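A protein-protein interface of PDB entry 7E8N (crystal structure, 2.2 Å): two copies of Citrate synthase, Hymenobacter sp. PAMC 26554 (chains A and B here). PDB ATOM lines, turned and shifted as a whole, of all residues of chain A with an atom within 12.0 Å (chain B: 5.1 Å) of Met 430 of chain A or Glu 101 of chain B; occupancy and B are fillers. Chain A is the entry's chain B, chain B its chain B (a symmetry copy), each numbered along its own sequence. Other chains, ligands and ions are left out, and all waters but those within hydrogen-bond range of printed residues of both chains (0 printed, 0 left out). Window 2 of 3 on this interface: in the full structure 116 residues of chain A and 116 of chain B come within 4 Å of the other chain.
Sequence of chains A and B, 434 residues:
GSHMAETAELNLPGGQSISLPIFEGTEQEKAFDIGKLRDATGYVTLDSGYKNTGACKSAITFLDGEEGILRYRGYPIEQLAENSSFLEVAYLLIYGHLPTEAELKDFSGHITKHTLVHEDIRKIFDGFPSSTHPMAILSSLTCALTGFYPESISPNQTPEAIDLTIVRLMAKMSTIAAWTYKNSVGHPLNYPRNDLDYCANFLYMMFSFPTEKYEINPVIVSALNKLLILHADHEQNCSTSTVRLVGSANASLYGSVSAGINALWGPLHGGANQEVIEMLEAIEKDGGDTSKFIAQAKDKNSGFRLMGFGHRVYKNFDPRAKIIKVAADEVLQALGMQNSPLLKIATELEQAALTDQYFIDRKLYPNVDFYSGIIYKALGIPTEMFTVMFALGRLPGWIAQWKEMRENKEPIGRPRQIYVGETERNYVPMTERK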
ATOM      1  N   ASN A 426       4.698   0.770   2.330  1.00  0.00           N
ATOM      2  CA  ASN A 426       3.280   0.477   2.572  1.00  0.00           C
ATOM      3  C   ASN A 426       3.219  -0.656   3.582  1.00  0.00           C
ATOM      4  O   ASN A 426       4.116  -1.520   3.538  1.00  0.00           O
ATOM      5  CB  ASN A 426       2.565   0.152   1.265  1.00  0.00           C
ATOM      6  CG  ASN A 426       2.426   1.367   0.380  1.00  0.00           C
ATOM      7  OD1 ASN A 426       1.957   2.418   0.824  1.00  0.00           O
ATOM      8  ND2 ASN A 426       2.827   1.224  -0.875  1.00  0.00           N
ATOM      9  N   TYR A 427       2.192  -0.635   4.427  1.00  0.00           N
ATOM     10  CA  TYR A 427       1.877  -1.697   5.420  1.00  0.00           C
ATOM     11  C   TYR A 427       1.946  -3.046   4.702  1.00  0.00           C
ATOM     12  O   TYR A 427       1.499  -3.099   3.557  1.00  0.00           O
ATOM     13  CB  TYR A 427       0.496  -1.463   6.033  1.00  0.00           C
ATOM     14  CG  TYR A 427       0.094  -2.408   7.134  1.00  0.00           C
ATOM     15  CD1 TYR A 427       0.551  -2.220   8.425  1.00  0.00           C
ATOM     16  CD2 TYR A 427      -0.754  -3.472   6.898  1.00  0.00           C
ATOM     17  CE1 TYR A 427       0.213  -3.076   9.450  1.00  0.00           C
ATOM     18  CE2 TYR A 427      -1.160  -4.311   7.924  1.00  0.00           C
ATOM     19  CZ  TYR A 427      -0.662  -4.116   9.204  1.00  0.00           C
ATOM     20  OH  TYR A 427      -1.015  -4.916  10.254  1.00  0.00           O
ATOM     21  N   VAL A 428       2.550  -4.057   5.331  1.00  0.00           N
ATOM     22  CA  VAL A 428       2.559  -5.470   4.854  1.00  0.00           C
ATOM     23  C   VAL A 428       1.561  -6.223   5.722  1.00  0.00           C
ATOM     24  O   VAL A 428       1.736  -6.315   6.937  1.00  0.00           O
ATOM     25  CB  VAL A 428       3.975  -6.079   4.928  1.00  0.00           C
ATOM     26  CG1 VAL A 428       4.036  -7.547   4.508  1.00  0.00           C
ATOM     27  CG2 VAL A 428       4.963  -5.289   4.087  1.00  0.00           C
ATOM     28  N   PRO A 429       0.472  -6.781   5.152  1.00  0.00           N
ATOM     29  CA  PRO A 429      -0.437  -7.610   5.936  1.00  0.00           C
ATOM     30  C   PRO A 429       0.352  -8.738   6.633  1.00  0.00           C
ATOM     31  O   PRO A 429       1.401  -9.190   6.095  1.00  0.00           O
ATOM     32  CB  PRO A 429      -1.410  -8.235   4.914  1.00  0.00           C
ATOM     33  CG  PRO A 429      -1.210  -7.445   3.634  1.00  0.00           C
ATOM     34  CD  PRO A 429       0.156  -6.794   3.719  1.00  0.00           C
ATOM     35  N   MET A 430      -0.149  -9.139   7.808  1.00  0.00           N
ATOM     36  CA  MET A 430       0.462 -10.115   8.734  1.00  0.00           C
ATOM     37  C   MET A 430       0.853 -11.409   7.983  1.00  0.00           C
ATOM     38  O   MET A 430       2.020 -11.836   8.071  1.00  0.00           O
ATOM     39  CB  MET A 430      -0.541 -10.424   9.847  1.00  0.00           C
ATOM     40  CG  MET A 430      -0.118 -11.601  10.703  1.00  0.00           C
ATOM     41  SD  MET A 430       1.486 -11.303  11.424  1.00  0.00           S
ATOM     42  CE  MET A 430       0.875 -10.416  12.861  1.00  0.00           C
ATOM     43  N   THR A 431      -0.065 -11.985   7.225  1.00  0.00           N
ATOM     44  CA  THR A 431       0.130 -13.272   6.504  1.00  0.00           C
ATOM     45  C   THR A 431       1.227 -13.166   5.433  1.00  0.00           C
ATOM     46  O   THR A 431       1.693 -14.224   5.019  1.00  0.00           O
ATOM     47  CB  THR A 431      -1.181 -13.761   5.890  1.00  0.00           C
ATOM     48  OG1 THR A 431      -1.696 -12.687   5.105  1.00  0.00           O
ATOM     49  CG2 THR A 431      -2.178 -14.178   6.952  1.00  0.00           C
ATOM     50  N   GLU A 432       1.663 -11.969   5.015  1.00  0.00           N
ATOM     51  CA  GLU A 432       2.690 -11.856   3.940  1.00  0.00           C
ATOM     52  C   GLU A 432       4.080 -11.591   4.519  1.00  0.00           C
ATOM     53  O   GLU A 432       5.024 -11.467   3.711  1.00  0.00           O
ATOM     54  CB  GLU A 432       2.340 -10.754   2.956  1.00  0.00           C
ATOM     55  CG  GLU A 432       1.139 -11.069   2.106  1.00  0.00           C
ATOM     56  CD  GLU A 432       0.607  -9.840   1.395  1.00  0.00           C
ATOM     57  OE1 GLU A 432       1.395  -8.888   1.211  1.00  0.00           O
ATOM     58  OE2 GLU A 432      -0.596  -9.825   1.063  1.00  0.00           O
ATOM     59  N   ARG A 433       4.208 -11.529   5.847  1.00  0.00           N
ATOM     60  CA  ARG A 433       5.494 -11.229   6.524  1.00  0.00           C
ATOM     61  C   ARG A 433       6.310 -12.519   6.676  1.00  0.00           C
ATOM     62  O   ARG A 433       5.778 -13.529   7.175  1.00  0.00           O
ATOM     63  CB  ARG A 433       5.202 -10.544   7.858  1.00  0.00           C
ATOM     64  CG  ARG A 433       4.536  -9.188   7.673  1.00  0.00           C
ATOM     65  CD  ARG A 433       4.182  -8.601   9.016  1.00  0.00           C
ATOM     66  NE  ARG A 433       3.044  -7.707   8.976  1.00  0.00           N
ATOM     67  CZ  ARG A 433       2.413  -7.239  10.048  1.00  0.00           C
ATOM     68  NH1 ARG A 433       2.807  -7.603  11.260  1.00  0.00           N
ATOM     69  NH2 ARG A 433       1.360  -6.446   9.897  1.00  0.00           N
ATOM     70  N   LYS A 434       7.576 -12.489   6.283  1.00  0.00           N
ATOM     71  CA  LYS A 434       8.461 -13.679   6.404  1.00  0.00           C
ATOM     72  C   LYS A 434       9.777 -13.236   7.055  1.00  0.00           C
ATOM     73  O   LYS A 434      10.055 -13.721   8.146  1.00  0.00           O
ATOM     74  CB  LYS A 434       8.644 -14.353   5.037  1.00  0.00           C
ATOM     75  CG  LYS A 434       9.671 -15.483   4.996  1.00  0.00           C
ATOM     76  CD  LYS A 434      10.812 -15.263   4.009  1.00  0.00           C
ATOM     77  CE  LYS A 434      11.499 -13.918   4.172  1.00  0.00           C
ATOM     78  NZ  LYS A 434      12.767 -13.830   3.410  1.00  0.00           N
ATOM     79  N   GLU B  88       1.581  -4.260  18.007  1.00  0.00           N
ATOM     80  CA  GLU B  88       2.244  -4.390  16.674  1.00  0.00           C
ATOM     81  C   GLU B  88       3.025  -3.102  16.390  1.00  0.00           C
ATOM     82  O   GLU B  88       4.216  -3.200  16.030  1.00  0.00           O
ATOM     83  CB  GLU B  88       1.245  -4.718  15.563  1.00  0.00           C
ATOM     84  CG  GLU B  88       1.915  -4.763  14.196  1.00  0.00           C
ATOM     85  CD  GLU B  88       0.978  -5.236  13.100  1.00  0.00           C
ATOM     86  OE1 GLU B  88       0.252  -4.400  12.515  1.00  0.00           O
ATOM     87  OE2 GLU B  88       0.924  -6.452  12.889  1.00  0.00           O
ATOM     88  N   PRO B  99       6.256  -7.261  12.931  1.00  0.00           N
ATOM     89  CA  PRO B  99       6.535  -8.605  13.406  1.00  0.00           C
ATOM     90  C   PRO B  99       5.811  -9.628  12.520  1.00  0.00           C
ATOM     91  O   PRO B  99       4.692  -9.375  12.092  1.00  0.00           O
ATOM     92  CB  PRO B  99       5.971  -8.620  14.825  1.00  0.00           C
ATOM     93  CG  PRO B  99       4.840  -7.587  14.781  1.00  0.00           C
ATOM     94  CD  PRO B  99       5.285  -6.550  13.774  1.00  0.00           C
ATOM     95  N   THR B 100       6.446 -10.783  12.334  1.00  0.00           N
ATOM     96  CA  THR B 100       5.772 -12.006  11.856  1.00  0.00           C
ATOM     97  C   THR B 100       4.723 -12.387  12.894  1.00  0.00           C
ATOM     98  O   THR B 100       4.758 -11.823  14.014  1.00  0.00           O
ATOM     99  CB  THR B 100       6.765 -13.161  11.680  1.00  0.00           C
ATOM    100  OG1 THR B 100       7.237 -13.517  12.977  1.00  0.00           O
ATOM    101  CG2 THR B 100       7.958 -12.776  10.835  1.00  0.00           C
ATOM    102  N   GLU B 101       3.852 -13.325  12.542  1.00  0.00           N
ATOM    103  CA  GLU B 101       2.751 -13.775  13.410  1.00  0.00           C
ATOM    104  C   GLU B 101       3.343 -14.355  14.705  1.00  0.00           C
ATOM    105  O   GLU B 101       2.757 -14.105  15.788  1.00  0.00           O
ATOM    106  CB  GLU B 101       1.861 -14.771  12.668  1.00  0.00           C
ATOM    107  CG  GLU B 101       0.607 -15.111  13.463  1.00  0.00           C
ATOM    108  CD  GLU B 101      -0.274 -16.202  12.874  1.00  0.00           C
ATOM    109  OE1 GLU B 101       0.232 -17.007  12.042  1.00  0.00           O
ATOM    110  OE2 GLU B 101      -1.468 -16.235  13.251  1.00  0.00           O
ATOM    111  N   ALA B 102       4.477 -15.043  14.606  1.00  0.00           N
ATOM    112  CA  ALA B 102       5.150 -15.736  15.717  1.00  0.00           C
ATOM    113  C   ALA B 102       5.818 -14.680  16.608  1.00  0.00           C
ATOM    114  O   ALA B 102       5.720 -14.808  17.828  1.00  0.00           O
ATOM    115  CB  ALA B 102       6.147 -16.746  15.188  1.00  0.00           C
ATOM    116  N   GLU B 103       6.458 -13.667  16.019  1.00  0.00           N
ATOM    117  CA  GLU B 103       7.108 -12.579  16.788  1.00  0.00           C
ATOM    118  C   GLU B 103       6.052 -11.819  17.600  1.00  0.00           C
ATOM    119  O   GLU B 103       6.254 -11.657  18.797  1.00  0.00           O
ATOM    120  CB  GLU B 103       7.857 -11.637  15.861  1.00  0.00           C
ATOM    121  CG  GLU B 103       9.135 -12.224  15.299  1.00  0.00           C
ATOM    122  CD  GLU B 103       9.743 -11.405  14.167  1.00  0.00           C
ATOM    123  OE1 GLU B 103       8.978 -10.743  13.411  1.00  0.00           O
ATOM    124  OE2 GLU B 103      10.979 -11.399  14.071  1.00  0.00           O
ATOM    125  N   LEU B 104       4.951 -11.406  16.989  1.00  0.00           N
ATOM    126  CA  LEU B 104       3.890 -10.647  17.698  1.00  0.00           C
ATOM    127  C   LEU B 104       3.281 -11.541  18.781  1.00  0.00           C
ATOM    128  O   LEU B 104       2.993 -11.018  19.865  1.00  0.00           O
ATOM    129  CB  LEU B 104       2.815 -10.161  16.728  1.00  0.00           C
ATOM    130  CG  LEU B 104       1.732  -9.280  17.344  1.00  0.00           C
ATOM    131  CD1 LEU B 104       2.321  -8.103  18.086  1.00  0.00           C
ATOM    132  CD2 LEU B 104       0.804  -8.796  16.251  1.00  0.00           C
ATOM    133  N   LYS B 105       3.095 -12.831  18.515  1.00  0.00           N
ATOM    134  CA  LYS B 105       2.469 -13.754  19.496  1.00  0.00           C
ATOM    135  C   LYS B 105       3.383 -13.934  20.729  1.00  0.00           C
ATOM    136  O   LYS B 105       2.847 -13.946  21.852  1.00  0.00           O
ATOM    137  CB  LYS B 105       2.126 -15.113  18.865  1.00  0.00           C
ATOM    138  CG  LYS B 105       1.725 -16.175  19.882  1.00  0.00           C
ATOM    139  CD  LYS B 105       1.323 -17.506  19.284  1.00  0.00           C
ATOM    140  CE  LYS B 105       0.421 -18.291  20.220  1.00  0.00           C
ATOM    141  NZ  LYS B 105       0.063 -19.621  19.677  1.00  0.00           N
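NH2 of Arg 433 of chain A sits at hydrogen-bond distance from OH of Tyr 427 of chain A (2.8 Å). N of Thr 100 of chain B is in hydrogen-bond range of OE1 of Glu 103 of chain B, at 2.8 Å. NE of Arg 433 of chain A is in hydrogen-bond range of O of Val 428 of chain A (2.8 Å).
OE2 of Glu 88 of chain B touches CE of Met 430 of chain A (3.96 Å). Pro 99 of chain B touches Met 430 of chain A (O to SD, 3.8 Å). Met 430 of chain A touches Thr 100 of chain B (SD to C, 3.7 Å). Met 430 of chain A touches Leu 104 of chain B (CE to CD2, 3.8 Å). Thr 100 of chain B touches Lys 434 of chain A.
OH of Tyr 427 of chain A is in hydrogen-bond range of OE1 of Glu 88 of chain B, 2.6 Å away. The guanidinium group (NH1) of Arg 433 of chain A is in salt-bridge range of the side-chain carboxylate (OE2) of Glu 88 of chain B, 2.7 Å away. The backbone NH (N) of Glu 101 of chain B lies within hydrogen-bond range of the side-chain sulfur (SD) of Met 430 of chain A. NH1 of Arg 433 of chain A lies within hydrogen-bond range of O of Pro 99 of chain B (2.7 Å).
Met 430 of chain A touches five residues of chain B. Glu 101 of chain B touches just one residue of chain A: Met 430. Pro 99 of chain B touches two residues of chain A. No residue of chain A comes within 4 Å of Glu 103 of chain B. Of chain A, only Met 430 comes within 4 Å of Leu 104 of chain B. No residue of chain A comes within 4 Å of Lys 105 of chain B. Printed residues of chain A within 4 Å of Glu 88 of chain B: Tyr 427 (2.6 Å), Met 430 (3.96 Å) and Arg 433 (2.7 Å). Of the printed residues of chain B, Lys 434 of chain A touches Thr 100. Printed residues of chain B within 4 Å of Arg 433 of chain A: Glu 88 (2.7 Å) and Pro 99 (2.7 Å). Printed residues of chain B within 4 Å of Tyr 427 of chain A: Glu 88 (2.6 Å). The nearest printed residue of chain B that does not touch Met 430 of chain A is Ala 102 of chain B (5.7 Å). The nearest printed residue of chain A that does not touch Glu 88 of chain B is Val 428 of chain A (6.0 Å).
No position is printed for both chains.
Of the 9 printed residues of chain A, 4 touch a printed residue of chain B. Hydrophobic or aromatic side chains of chain A within 4 Å of the printed part of chain B: Tyr 427 and Met 430. Of the 8 printed residues of chain B, 5 touch a printed residue of chain A. Printed residues of chain B that touch a printed residue of chain A: Glu 88, Pro 99, Thr 100, Glu 101 and Leu 104. Hydrophobic or aromatic side chains of chain B that line the printed part of chain A: Pro 99 and Leu 104.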
